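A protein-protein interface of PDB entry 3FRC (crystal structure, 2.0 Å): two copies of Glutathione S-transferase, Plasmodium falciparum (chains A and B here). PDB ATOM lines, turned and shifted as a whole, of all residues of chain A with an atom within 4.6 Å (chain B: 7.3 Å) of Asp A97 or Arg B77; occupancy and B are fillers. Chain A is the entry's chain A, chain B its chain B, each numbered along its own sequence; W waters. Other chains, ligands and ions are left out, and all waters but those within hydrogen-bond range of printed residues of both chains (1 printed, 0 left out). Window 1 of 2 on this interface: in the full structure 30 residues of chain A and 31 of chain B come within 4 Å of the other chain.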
ATOM      1  N   ARG A  77       7.741 -18.131 -26.594  1.00  0.00           N
ATOM      2  CA  ARG A  77       8.274 -17.083 -25.723  1.00  0.00           C
ATOM      3  C   ARG A  77       9.509 -17.578 -24.978  1.00  0.00           C
ATOM      4  O   ARG A  77      10.499 -16.861 -24.873  1.00  0.00           O
ATOM      5  CB  ARG A  77       7.213 -16.565 -24.742  1.00  0.00           C
ATOM      6  CG  ARG A  77       6.244 -15.566 -25.373  1.00  0.00           C
ATOM      7  CD  ARG A  77       5.228 -15.044 -24.373  1.00  0.00           C
ATOM      8  NE  ARG A  77       4.213 -16.041 -24.026  1.00  0.00           N
ATOM      9  CZ  ARG A  77       3.122 -16.294 -24.746  1.00  0.00           C
ATOM     10  NH1 ARG A  77       2.895 -15.637 -25.867  1.00  0.00           N
ATOM     11  NH2 ARG A  77       2.254 -17.209 -24.332  1.00  0.00           N
ATOM     12  N   GLU A  93       9.922  -5.977 -25.680  1.00  0.00           N
ATOM     13  CA  GLU A  93       9.361  -7.307 -25.436  1.00  0.00           C
ATOM     14  C   GLU A  93       7.831  -7.256 -25.327  1.00  0.00           C
ATOM     15  O   GLU A  93       7.143  -8.164 -25.805  1.00  0.00           O
ATOM     16  CB  GLU A  93      10.008  -7.984 -24.216  1.00  0.00           C
ATOM     17  CG  GLU A  93       9.514  -9.422 -23.901  1.00  0.00           C
ATOM     18  CD  GLU A  93       9.295 -10.316 -25.141  1.00  0.00           C
ATOM     19  OE1 GLU A  93      10.092 -10.242 -26.108  1.00  0.00           O
ATOM     20  OE2 GLU A  93       8.317 -11.103 -25.141  1.00  0.00           O
ATOM     21  N   PHE A  94       7.298  -6.198 -24.724  1.00  0.00           N
ATOM     22  CA  PHE A  94       5.849  -6.025 -24.734  1.00  0.00           C
ATOM     23  C   PHE A  94       5.308  -5.959 -26.162  1.00  0.00           C
ATOM     24  O   PHE A  94       4.321  -6.616 -26.480  1.00  0.00           O
ATOM     25  CB  PHE A  94       5.357  -4.786 -23.975  1.00  0.00           C
ATOM     26  CG  PHE A  94       3.892  -4.516 -24.216  1.00  0.00           C
ATOM     27  CD1 PHE A  94       2.923  -5.258 -23.551  1.00  0.00           C
ATOM     28  CD2 PHE A  94       3.485  -3.595 -25.179  1.00  0.00           C
ATOM     29  CE1 PHE A  94       1.570  -5.054 -23.805  1.00  0.00           C
ATOM     30  CE2 PHE A  94       2.139  -3.391 -25.444  1.00  0.00           C
ATOM     31  CZ  PHE A  94       1.179  -4.117 -24.748  1.00  0.00           C
ATOM     32  N   TYR A  95       5.936  -5.138 -27.003  1.00  0.00           N
ATOM     33  CA  TYR A  95       5.432  -4.923 -28.355  1.00  0.00           C
ATOM     34  C   TYR A  95       5.486  -6.184 -29.203  1.00  0.00           C
ATOM     35  O   TYR A  95       4.554  -6.470 -29.948  1.00  0.00           O
ATOM     36  CB  TYR A  95       6.171  -3.786 -29.064  1.00  0.00           C
ATOM     37  CG  TYR A  95       5.797  -2.412 -28.578  1.00  0.00           C
ATOM     38  CD1 TYR A  95       6.779  -1.495 -28.231  1.00  0.00           C
ATOM     39  CD2 TYR A  95       4.459  -2.026 -28.459  1.00  0.00           C
ATOM     40  CE1 TYR A  95       6.449  -0.226 -27.780  1.00  0.00           C
ATOM     41  CE2 TYR A  95       4.119  -0.750 -28.002  1.00  0.00           C
ATOM     42  CZ  TYR A  95       5.124   0.138 -27.661  1.00  0.00           C
ATOM     43  OH  TYR A  95       4.819   1.411 -27.221  1.00  0.00           O
ATOM     44  N   ALA A  96       6.580  -6.932 -29.084  1.00  0.00           N
ATOM     45  CA  ALA A  96       6.708  -8.213 -29.775  1.00  0.00           C
ATOM     46  C   ALA A  96       5.590  -9.161 -29.337  1.00  0.00           C
ATOM     47  O   ALA A  96       4.984  -9.844 -30.161  1.00  0.00           O
ATOM     48  CB  ALA A  96       8.079  -8.826 -29.505  1.00  0.00           C
ATOM     49  N   ASP A  97       5.323  -9.167 -28.033  1.00  0.00           N
ATOM     50  CA  ASP A  97       4.276  -9.978 -27.420  1.00  0.00           C
ATOM     51  C   ASP A  97       2.904  -9.580 -27.960  1.00  0.00           C
ATOM     52  O   ASP A  97       2.112 -10.433 -28.367  1.00  0.00           O
ATOM     53  CB  ASP A  97       4.322  -9.789 -25.899  1.00  0.00           C
ATOM     54  CG  ASP A  97       3.615 -10.893 -25.136  1.00  0.00           C
ATOM     55  OD1 ASP A  97       2.913 -11.731 -25.754  1.00  0.00           O
ATOM     56  OD2 ASP A  97       3.779 -10.924 -23.896  1.00  0.00           O
ATOM     57  N   MET A  98       2.648  -8.276 -27.955  1.00  0.00           N
ATOM     58  CA  MET A  98       1.391  -7.724 -28.446  1.00  0.00           C
ATOM     59  C   MET A  98       1.128  -8.121 -29.895  1.00  0.00           C
ATOM     60  O   MET A  98       0.019  -8.513 -30.245  1.00  0.00           O
ATOM     61  CB  MET A  98       1.392  -6.203 -28.300  1.00  0.00           C
ATOM     62  CG  MET A  98       0.102  -5.529 -28.735  1.00  0.00           C
ATOM     63  SD  MET A  98       0.289  -3.743 -28.817  1.00  0.00           S
ATOM     64  CE  MET A  98       0.990  -3.520 -30.456  1.00  0.00           C
ATOM     65  N   ILE A  99       2.157  -8.024 -30.731  1.00  0.00           N
ATOM     66  CA  ILE A  99       2.047  -8.374 -32.152  1.00  0.00           C
ATOM     67  C   ILE A  99       1.810  -9.875 -32.351  1.00  0.00           C
ATOM     68  O   ILE A  99       1.007 -10.284 -33.193  1.00  0.00           O
ATOM     69  CB  ILE A  99       3.293  -7.866 -32.936  1.00  0.00           C
ATOM     70  CG1 ILE A  99       3.244  -6.336 -33.012  1.00  0.00           C
ATOM     71  CG2 ILE A  99       3.360  -8.490 -34.331  1.00  0.00           C
ATOM     72  CD1 ILE A  99       4.560  -5.645 -33.407  1.00  0.00           C
ATOM     73  N   PHE A 100       2.501 -10.684 -31.558  1.00  0.00           N
ATOM     74  CA  PHE A 100       2.297 -12.129 -31.547  1.00  0.00           C
ATOM     75  C   PHE A 100       0.848 -12.463 -31.152  1.00  0.00           C
ATOM     76  O   PHE A 100       0.213 -13.330 -31.750  1.00  0.00           O
ATOM     77  CB  PHE A 100       3.323 -12.781 -30.606  1.00  0.00           C
ATOM     78  CG  PHE A 100       3.285 -14.290 -30.584  1.00  0.00           C
ATOM     79  CD1 PHE A 100       2.982 -15.020 -31.720  1.00  0.00           C
ATOM     80  CD2 PHE A 100       3.585 -14.979 -29.416  1.00  0.00           C
ATOM     81  CE1 PHE A 100       2.958 -16.415 -31.688  1.00  0.00           C
ATOM     82  CE2 PHE A 100       3.561 -16.368 -29.374  1.00  0.00           C
ATOM     83  CZ  PHE A 100       3.249 -17.083 -30.511  1.00  0.00           C
ATOM     84  N   CYS A 101       0.327 -11.743 -30.168  1.00  0.00           N
ATOM     85  CA  CYS A 101      -1.067 -11.886 -29.760  1.00  0.00           C
ATOM     86  C   CYS A 101      -2.038 -11.486 -30.872  1.00  0.00           C
ATOM     87  O   CYS A 101      -3.060 -12.147 -31.074  1.00  0.00           O
ATOM     88  CB  CYS A 101      -1.321 -11.074 -28.499  1.00  0.00           C
ATOM     89  SG  CYS A 101      -0.528 -11.785 -27.060  1.00  0.00           S
ATOM     90  N   TYR A 160      10.850 -12.761 -32.432  1.00  0.00           N
ATOM     91  CA  TYR A 160       9.923 -13.840 -32.764  1.00  0.00           C
ATOM     92  C   TYR A 160       8.641 -13.319 -33.412  1.00  0.00           C
ATOM     93  O   TYR A 160       7.979 -14.058 -34.142  1.00  0.00           O
ATOM     94  CB  TYR A 160       9.607 -14.702 -31.541  1.00  0.00           C
ATOM     95  CG  TYR A 160       8.848 -14.003 -30.438  1.00  0.00           C
ATOM     96  CD1 TYR A 160       7.461 -14.158 -30.313  1.00  0.00           C
ATOM     97  CD2 TYR A 160       9.508 -13.207 -29.502  1.00  0.00           C
ATOM     98  CE1 TYR A 160       6.759 -13.531 -29.295  1.00  0.00           C
ATOM     99  CE2 TYR A 160       8.804 -12.572 -28.475  1.00  0.00           C
ATOM    100  CZ  TYR A 160       7.431 -12.746 -28.380  1.00  0.00           C
ATOM    101  OH  TYR A 160       6.730 -12.131 -27.369  1.00  0.00           O
ATOM    102  N   ILE B  22      -5.254  -8.193 -11.286  1.00  0.00           N
ATOM    103  CA  ILE B  22      -3.833  -7.950 -11.118  1.00  0.00           C
ATOM    104  C   ILE B  22      -3.553  -6.582 -10.482  1.00  0.00           C
ATOM    105  O   ILE B  22      -2.695  -6.462  -9.607  1.00  0.00           O
ATOM    106  CB  ILE B  22      -3.083  -8.165 -12.468  1.00  0.00           C
ATOM    107  CG1 ILE B  22      -3.028  -9.668 -12.769  1.00  0.00           C
ATOM    108  CG2 ILE B  22      -1.665  -7.585 -12.420  1.00  0.00           C
ATOM    109  CD1 ILE B  22      -2.573 -10.032 -14.183  1.00  0.00           C
ATOM    110  N   PHE B  56      -5.062  -2.566 -33.075  1.00  0.00           N
ATOM    111  CA  PHE B  56      -5.960  -3.573 -33.668  1.00  0.00           C
ATOM    112  C   PHE B  56      -7.457  -3.267 -33.532  1.00  0.00           C
ATOM    113  O   PHE B  56      -8.288  -4.142 -33.753  1.00  0.00           O
ATOM    114  CB  PHE B  56      -5.689  -4.971 -33.082  1.00  0.00           C
ATOM    115  CG  PHE B  56      -4.244  -5.397 -33.144  1.00  0.00           C
ATOM    116  CD1 PHE B  56      -3.540  -5.663 -31.978  1.00  0.00           C
ATOM    117  CD2 PHE B  56      -3.594  -5.538 -34.368  1.00  0.00           C
ATOM    118  CE1 PHE B  56      -2.218  -6.053 -32.023  1.00  0.00           C
ATOM    119  CE2 PHE B  56      -2.268  -5.937 -34.425  1.00  0.00           C
ATOM    120  CZ  PHE B  56      -1.578  -6.193 -33.256  1.00  0.00           C
ATOM    121  N   ALA B  70      -1.978  -2.673 -25.941  1.00  0.00           N
ATOM    122  CA  ALA B  70      -3.087  -3.537 -26.338  1.00  0.00           C
ATOM    123  C   ALA B  70      -2.771  -5.006 -26.119  1.00  0.00           C
ATOM    124  O   ALA B  70      -1.623  -5.370 -25.824  1.00  0.00           O
ATOM    125  CB  ALA B  70      -3.467  -3.294 -27.809  1.00  0.00           C
ATOM    126  N   GLN B  71      -3.802  -5.833 -26.299  1.00  0.00           N
ATOM    127  CA  GLN B  71      -3.755  -7.296 -26.175  1.00  0.00           C
ATOM    128  C   GLN B  71      -3.676  -7.766 -24.728  1.00  0.00           C
ATOM    129  O   GLN B  71      -2.618  -7.719 -24.103  1.00  0.00           O
ATOM    130  CB  GLN B  71      -2.655  -7.919 -27.047  1.00  0.00           C
ATOM    131  CG  GLN B  71      -2.942  -7.850 -28.550  1.00  0.00           C
ATOM    132  CD  GLN B  71      -4.018  -8.821 -29.014  1.00  0.00           C
ATOM    133  OE1 GLN B  71      -4.441  -9.711 -28.274  1.00  0.00           O
ATOM    134  NE2 GLN B  71      -4.454  -8.664 -30.260  1.00  0.00           N
ATOM    135  N   SER B  72      -4.818  -8.230 -24.215  1.00  0.00           N
ATOM    136  CA  SER B  72      -4.970  -8.583 -22.801  1.00  0.00           C
ATOM    137  C   SER B  72      -3.875  -9.503 -22.263  1.00  0.00           C
ATOM    138  O   SER B  72      -3.375  -9.274 -21.170  1.00  0.00           O
ATOM    139  CB  SER B  72      -6.347  -9.198 -22.540  1.00  0.00           C
ATOM    140  OG  SER B  72      -6.522 -10.373 -23.308  1.00  0.00           O
ATOM    141  N   GLN B  73      -3.509 -10.533 -23.034  1.00  0.00           N
ATOM    142  CA  GLN B  73      -2.438 -11.471 -22.649  1.00  0.00           C
ATOM    143  C   GLN B  73      -1.068 -10.815 -22.534  1.00  0.00           C
ATOM    144  O   GLN B  73      -0.296 -11.121 -21.620  1.00  0.00           O
ATOM    145  CB  GLN B  73      -2.302 -12.572 -23.691  1.00  0.00           C
ATOM    146  CG  GLN B  73      -3.297 -13.694 -23.639  1.00  0.00           C
ATOM    147  CD  GLN B  73      -2.858 -14.850 -24.528  1.00  0.00           C
ATOM    148  OE1 GLN B  73      -1.668 -15.233 -24.553  1.00  0.00           O
ATOM    149  NE2 GLN B  73      -3.809 -15.410 -25.268  1.00  0.00           N
ATOM    150  N   ALA B  74      -0.752  -9.951 -23.499  1.00  0.00           N
ATOM    151  CA  ALA B  74       0.500  -9.211 -23.495  1.00  0.00           C
ATOM    152  C   ALA B  74       0.559  -8.270 -22.301  1.00  0.00           C
ATOM    153  O   ALA B  74       1.592  -8.169 -21.635  1.00  0.00           O
ATOM    154  CB  ALA B  74       0.667  -8.449 -24.790  1.00  0.00           C
ATOM    155  N   ILE B  75      -0.558  -7.604 -22.022  1.00  0.00           N
ATOM    156  CA  ILE B  75      -0.666  -6.695 -20.877  1.00  0.00           C
ATOM    157  C   ILE B  75      -0.476  -7.473 -19.572  1.00  0.00           C
ATOM    158  O   ILE B  75       0.304  -7.066 -18.698  1.00  0.00           O
ATOM    159  CB  ILE B  75      -2.025  -5.918 -20.877  1.00  0.00           C
ATOM    160  CG1 ILE B  75      -2.089  -4.936 -22.061  1.00  0.00           C
ATOM    161  CG2 ILE B  75      -2.223  -5.174 -19.553  1.00  0.00           C
ATOM    162  CD1 ILE B  75      -3.491  -4.499 -22.468  1.00  0.00           C
ATOM    163  N   VAL B  76      -1.180  -8.596 -19.444  1.00  0.00           N
ATOM    164  CA  VAL B  76      -1.005  -9.476 -18.285  1.00  0.00           C
ATOM    165  C   VAL B  76       0.462  -9.852 -18.072  1.00  0.00           C
ATOM    166  O   VAL B  76       0.993  -9.698 -16.965  1.00  0.00           O
ATOM    167  CB  VAL B  76      -1.900 -10.740 -18.389  1.00  0.00           C
ATOM    168  CG1 VAL B  76      -1.451 -11.814 -17.413  1.00  0.00           C
ATOM    169  CG2 VAL B  76      -3.362 -10.373 -18.104  1.00  0.00           C
ATOM    170  N   ARG B  77       1.119 -10.337 -19.125  1.00  0.00           N
ATOM    171  CA  ARG B  77       2.512 -10.760 -19.017  1.00  0.00           C
ATOM    172  C   ARG B  77       3.436  -9.599 -18.693  1.00  0.00           C
ATOM    173  O   ARG B  77       4.371  -9.747 -17.915  1.00  0.00           O
ATOM    174  CB  ARG B  77       2.974 -11.493 -20.281  1.00  0.00           C
ATOM    175  CG  ARG B  77       2.617 -12.969 -20.288  1.00  0.00           C
ATOM    176  CD  ARG B  77       3.118 -13.663 -21.564  1.00  0.00           C
ATOM    177  NE  ARG B  77       2.450 -13.173 -22.773  1.00  0.00           N
ATOM    178  CZ  ARG B  77       1.314 -13.671 -23.262  1.00  0.00           C
ATOM    179  NH1 ARG B  77       0.696 -14.672 -22.647  1.00  0.00           N
ATOM    180  NH2 ARG B  77       0.793 -13.164 -24.368  1.00  0.00           N
ATOM    181  N   TYR B  78       3.148  -8.440 -19.278  1.00  0.00           N
ATOM    182  CA  TYR B  78       3.937  -7.238 -19.042  1.00  0.00           C
ATOM    183  C   TYR B  78       3.903  -6.830 -17.574  1.00  0.00           C
ATOM    184  O   TYR B  78       4.946  -6.549 -16.972  1.00  0.00           O
ATOM    185  CB  TYR B  78       3.439  -6.102 -19.942  1.00  0.00           C
ATOM    186  CG  TYR B  78       4.030  -4.742 -19.645  1.00  0.00           C
ATOM    187  CD1 TYR B  78       5.313  -4.414 -20.072  1.00  0.00           C
ATOM    188  CD2 TYR B  78       3.303  -3.784 -18.936  1.00  0.00           C
ATOM    189  CE1 TYR B  78       5.864  -3.164 -19.804  1.00  0.00           C
ATOM    190  CE2 TYR B  78       3.842  -2.527 -18.660  1.00  0.00           C
ATOM    191  CZ  TYR B  78       5.125  -2.227 -19.105  1.00  0.00           C
ATOM    192  OH  TYR B  78       5.675  -0.986 -18.851  1.00  0.00           O
ATOM    193  N   LEU B  79       2.700  -6.805 -17.002  1.00  0.00           N
ATOM    194  CA  LEU B  79       2.520  -6.414 -15.608  1.00  0.00           C
ATOM    195  C   LEU B  79       3.129  -7.419 -14.635  1.00  0.00           C
ATOM    196  O   LEU B  79       3.778  -7.035 -13.657  1.00  0.00           O
ATOM    197  CB  LEU B  79       1.032  -6.226 -15.302  1.00  0.00           C
ATOM    198  CG  LEU B  79       0.350  -5.050 -16.000  1.00  0.00           C
ATOM    199  CD1 LEU B  79      -1.161  -5.160 -15.824  1.00  0.00           C
ATOM    200  CD2 LEU B  79       0.891  -3.708 -15.489  1.00  0.00           C
ATOM    201  N   SER B  80       2.909  -8.703 -14.906  1.00  0.00           N
ATOM    202  CA  SER B  80       3.379  -9.777 -14.027  1.00  0.00           C
ATOM    203  C   SER B  80       4.897  -9.842 -13.955  1.00  0.00           C
ATOM    204  O   SER B  80       5.470 -10.120 -12.891  1.00  0.00           O
ATOM    205  CB  SER B  80       2.820 -11.121 -14.489  1.00  0.00           C
ATOM    206  OG  SER B  80       1.411 -11.049 -14.576  1.00  0.00           O
ATOM    207  N   LYS B  81       5.543  -9.588 -15.085  1.00  0.00           N
ATOM    208  CA  LYS B  81       6.997  -9.533 -15.154  1.00  0.00           C
ATOM    209  C   LYS B  81       7.527  -8.319 -14.382  1.00  0.00           C
ATOM    210  O   LYS B  81       8.495  -8.419 -13.623  1.00  0.00           O
ATOM    211  CB  LYS B  81       7.443  -9.486 -16.624  1.00  0.00           C
ATOM    212  CG  LYS B  81       8.943  -9.561 -16.858  1.00  0.00           C
ATOM    213  CD  LYS B  81       9.518 -10.915 -16.461  1.00  0.00           C
ATOM    214  CE  LYS B  81      10.991 -11.045 -16.837  1.00  0.00           C
ATOM    215  NZ  LYS B  81      11.182 -11.696 -18.171  1.00  0.00           N
ATOM    216  N   LYS B  82       6.866  -7.180 -14.568  1.00  0.00           N
ATOM    217  CA  LYS B  82       7.271  -5.916 -13.954  1.00  0.00           C
ATOM    218  C   LYS B  82       7.175  -5.958 -12.427  1.00  0.00           C
ATOM    219  O   LYS B  82       8.021  -5.388 -11.729  1.00  0.00           O
ATOM    220  CB  LYS B  82       6.405  -4.780 -14.514  1.00  0.00           C
ATOM    221  CG  LYS B  82       6.849  -3.391 -14.119  1.00  0.00           C
ATOM    222  CD  LYS B  82       6.129  -2.320 -14.932  1.00  0.00           C
ATOM    223  CE  LYS B  82       6.829  -0.972 -14.775  1.00  0.00           C
ATOM    224  NZ  LYS B  82       8.100  -0.914 -15.564  1.00  0.00           N
ATOM    225  N   TYR B  83       6.148  -6.638 -11.923  1.00  0.00           N
ATOM    226  CA  TYR B  83       5.872  -6.700 -10.487  1.00  0.00           C
ATOM    227  C   TYR B  83       6.120  -8.078  -9.865  1.00  0.00           C
ATOM    228  O   TYR B  83       5.556  -8.400  -8.813  1.00  0.00           O
ATOM    229  CB  TYR B  83       4.436  -6.260 -10.213  1.00  0.00           C
ATOM    230  CG  TYR B  83       4.194  -4.785 -10.391  1.00  0.00           C
ATOM    231  CD1 TYR B  83       4.387  -3.896  -9.336  1.00  0.00           C
ATOM    232  CD2 TYR B  83       3.756  -4.279 -11.608  1.00  0.00           C
ATOM    233  CE1 TYR B  83       4.162  -2.532  -9.496  1.00  0.00           C
ATOM    234  CE2 TYR B  83       3.531  -2.925 -11.783  1.00  0.00           C
ATOM    235  CZ  TYR B  83       3.735  -2.058 -10.723  1.00  0.00           C
ATOM    236  OH  TYR B  83       3.503  -0.715 -10.898  1.00  0.00           O
ATOM    237  N   CYS B  86       5.482 -13.617 -12.064  1.00  0.00           N
ATOM    238  CA  CYS B  86       5.554 -14.453 -13.261  1.00  0.00           C
ATOM    239  C   CYS B  86       6.305 -15.766 -13.015  1.00  0.00           C
ATOM    240  O   CYS B  86       6.406 -16.597 -13.907  1.00  0.00           O
ATOM    241  CB  CYS B  86       6.193 -13.673 -14.417  1.00  0.00           C
ATOM    242  SG  CYS B  86       7.825 -13.056 -14.030  1.00  0.00           S
ATOM    243  N   GLU B  93       8.801 -19.388 -14.811  1.00  0.00           N
ATOM    244  CA  GLU B  93       8.207 -18.405 -15.697  1.00  0.00           C
ATOM    245  C   GLU B  93       7.582 -19.094 -16.910  1.00  0.00           C
ATOM    246  O   GLU B  93       6.470 -18.751 -17.297  1.00  0.00           O
ATOM    247  CB  GLU B  93       9.235 -17.355 -16.114  1.00  0.00           C
ATOM    248  CG  GLU B  93       8.688 -16.257 -17.000  1.00  0.00           C
ATOM    249  CD  GLU B  93       9.620 -15.072 -17.088  1.00  0.00           C
ATOM    250  OE1 GLU B  93      10.578 -14.996 -16.292  1.00  0.00           O
ATOM    251  OE2 GLU B  93       9.397 -14.208 -17.952  1.00  0.00           O
ATOM    252  N   ASP B  97       3.491 -19.461 -17.774  1.00  0.00           N
ATOM    253  CA  ASP B  97       3.059 -19.131 -19.131  1.00  0.00           C
ATOM    254  C   ASP B  97       2.245 -20.280 -19.723  1.00  0.00           C
ATOM    255  O   ASP B  97       1.195 -20.067 -20.314  1.00  0.00           O
ATOM    256  CB  ASP B  97       4.288 -18.849 -20.004  1.00  0.00           C
ATOM    257  CG  ASP B  97       3.945 -18.154 -21.306  1.00  0.00           C
ATOM    258  OD1 ASP B  97       2.762 -18.157 -21.711  1.00  0.00           O
ATOM    259  OD2 ASP B  97       4.869 -17.601 -21.932  1.00  0.00           O
ATOM    260  N   PHE B 100      -1.253 -20.423 -18.039  1.00  0.00           N
ATOM    261  CA  PHE B 100      -2.079 -19.325 -18.557  1.00  0.00           C
ATOM    262  C   PHE B 100      -2.561 -19.608 -19.990  1.00  0.00           C
ATOM    263  O   PHE B 100      -3.708 -19.344 -20.324  1.00  0.00           O
ATOM    264  CB  PHE B 100      -1.312 -18.001 -18.488  1.00  0.00           C
ATOM    265  CG  PHE B 100      -2.123 -16.796 -18.905  1.00  0.00           C
ATOM    266  CD1 PHE B 100      -3.319 -16.482 -18.270  1.00  0.00           C
ATOM    267  CD2 PHE B 100      -1.683 -15.969 -19.925  1.00  0.00           C
ATOM    268  CE1 PHE B 100      -4.064 -15.361 -18.657  1.00  0.00           C
ATOM    269  CE2 PHE B 100      -2.424 -14.850 -20.314  1.00  0.00           C
ATOM    270  CZ  PHE B 100      -3.613 -14.552 -19.683  1.00  0.00           C
ATOM    271  N   CYS B 101      -1.684 -20.155 -20.829  1.00  0.00           N
ATOM    272  CA  CYS B 101      -2.083 -20.551 -22.179  1.00  0.00           C
ATOM    273  C   CYS B 101      -3.176 -21.624 -22.157  1.00  0.00           C
ATOM    274  O   CYS B 101      -4.075 -21.604 -22.989  1.00  0.00           O
ATOM    275  CB  CYS B 101      -0.876 -21.002 -22.997  1.00  0.00           C
ATOM    276  SG  CYS B 101       0.208 -19.646 -23.462  1.00  0.00           S
ATOM    277  N   GLN B 104      -6.412 -20.103 -21.324  1.00  0.00           N
ATOM    278  CA  GLN B 104      -6.955 -19.463 -22.526  1.00  0.00           C
ATOM    279  C   GLN B 104      -7.748 -20.438 -23.407  1.00  0.00           C
ATOM    280  O   GLN B 104      -8.805 -20.082 -23.918  1.00  0.00           O
ATOM    281  CB  GLN B 104      -5.864 -18.753 -23.335  1.00  0.00           C
ATOM    282  CG  GLN B 104      -5.073 -17.687 -22.556  1.00  0.00           C
ATOM    283  CD  GLN B 104      -5.965 -16.676 -21.835  1.00  0.00           C
ATOM    284  OE1 GLN B 104      -6.591 -15.822 -22.463  1.00  0.00           O
ATOM    285  NE2 GLN B 104      -6.022 -16.773 -20.508  1.00  0.00           N
ATOM    286  N   TYR B 160       0.696 -14.964 -11.727  1.00  0.00           N
ATOM    287  CA  TYR B 160      -0.472 -14.566 -12.498  1.00  0.00           C
ATOM    288  C   TYR B 160      -1.258 -15.775 -12.999  1.00  0.00           C
ATOM    289  O   TYR B 160      -2.431 -15.645 -13.329  1.00  0.00           O
ATOM    290  CB  TYR B 160      -0.077 -13.635 -13.650  1.00  0.00           C
ATOM    291  CG  TYR B 160       0.654 -14.295 -14.793  1.00  0.00           C
ATOM    292  CD1 TYR B 160      -0.033 -14.700 -15.942  1.00  0.00           C
ATOM    293  CD2 TYR B 160       2.030 -14.494 -14.745  1.00  0.00           C
ATOM    294  CE1 TYR B 160       0.625 -15.297 -17.002  1.00  0.00           C
ATOM    295  CE2 TYR B 160       2.704 -15.096 -15.815  1.00  0.00           C
ATOM    296  CZ  TYR B 160       1.991 -15.494 -16.934  1.00  0.00           C
ATOM    297  OH  TYR B 160       2.644 -16.081 -17.995  1.00  0.00           O
HETATM  298  O   HOH W   1       3.954  -8.637 -22.720  1.00  0.00           O
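SG of Cys A101 sits at hydrogen-bond distance from NH2 of Arg B77.
OD2 of Asp A97 is in salt-bridge range of NE of Arg B77 (2.8 Å).
The side-chain carboxylate (OD2) of Asp B97 lies within salt-bridge range of the guanidinium group (NE) of Arg A77 (2.7 Å).
The guanidinium group (NH2) of Arg A77 lies close to the guanidinium group (NH1) of Arg B77, at 3.4 Å.
The guanidinium group (NH2) of Arg A77 is in hydrogen-bond range of the side-chain sulfur (SG) of Cys B101, 3.3 Å away.
The backbone carbonyl oxygen of Asp A97 lies within hydrogen-bond range of the side-chain sulfur of Cys A101 (3.2 Å).
O of Asp B97 sits at hydrogen-bond distance from SG of Cys B101 (3.3 Å).
The side-chain hydroxyl (OH) of Tyr A160 sits close to the backbone NH (N) of Asp A97 (3.3 Å).
OE1 of Gln B73 sits at hydrogen-bond distance from NH1 of Arg B77, 3.1 Å away.
N of Asp B97 lies close to OH of Tyr B160 (3.5 Å).
The guanidinium group (NH1) of Arg A77 is in salt-bridge range of the side-chain carboxylate (OD1) of Asp A97.
Among the printed residues, merely in contact across the chains: Phe A94 with Ala B70 (3.3 Å), Phe A94 with Ala B74 (3.6 Å), Phe A94 with Ile B75 (3.8 Å), Phe A94 with Tyr B78 (3.7 Å), Asp A97 with Ala B74 (3.7 Å), Met A98 with Phe B56 (3.8 Å), Met A98 with Ala B70 (3.4 Å), Met A98 with Gln B71 (3.5 Å), Met A98 with Ala B74 (3.7 Å), Cys A101 with Gln B71 (3.4 Å) and Cys A101 with Gln B73 (3.9 Å).
Asp A97 touches just these residues of chain B: Ala B74 (3.7 Å) and Arg B77 (2.8 Å).
Of chain A, only Arg A77, Asp A97 and Cys A101 come within 4 Å of Arg B77.
No residue of chain B comes within 4 Å of Ala A96.
Of the printed residues of chain A, Gln B73 touches Cys A101.
Printed residues of chain A within 4 Å of Ala B70: Phe A94 (3.3 Å) and Met A98 (3.4 Å).
Printed residues of chain A within 4 Å of Asp B97: Arg A77.
Printed residues of chain B within 4 Å of Phe A94: Ala B70, Ala B74, Ile B75 and Tyr B78.
The nearest printed residue of chain A that does not touch Arg B77 is Phe A100 (6.0 Å).
The nearest printed residue of chain A that does not touch Ala B70 is Cys A101 (6.3 Å).
Of the 23 printed residues of chain B, 10 touch a printed residue of chain A.
Printed residues of chain A that touch a printed residue of chain B: Arg A77, Phe A94, Asp A97, Met A98 and Cys A101.
Among the printed residues, Asp or Glu carboxylates within 4 Å of a Lys or Arg side-chain nitrogen of the other chain: Arg A77 with Asp B97 (2.7 Å) and Asp A97 with Arg B77 (2.8 Å).
Arg B77 touches its own counterpart, Arg A77.
Arg A77 touches Asp B97, and with the chains exchanged Asp A97 touches Arg B77.
Arg A77 touches Cys B101, and with the chains exchanged Cys A101 touches Arg B77.
Of the 16 pairs that touch across the chains among the printed residues, 5 have their exchanged pair printed and touching as well.
Water W1 bridges OD2 of Asp A97 (2.6 Å) and O of Ala B74 (2.6 Å).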
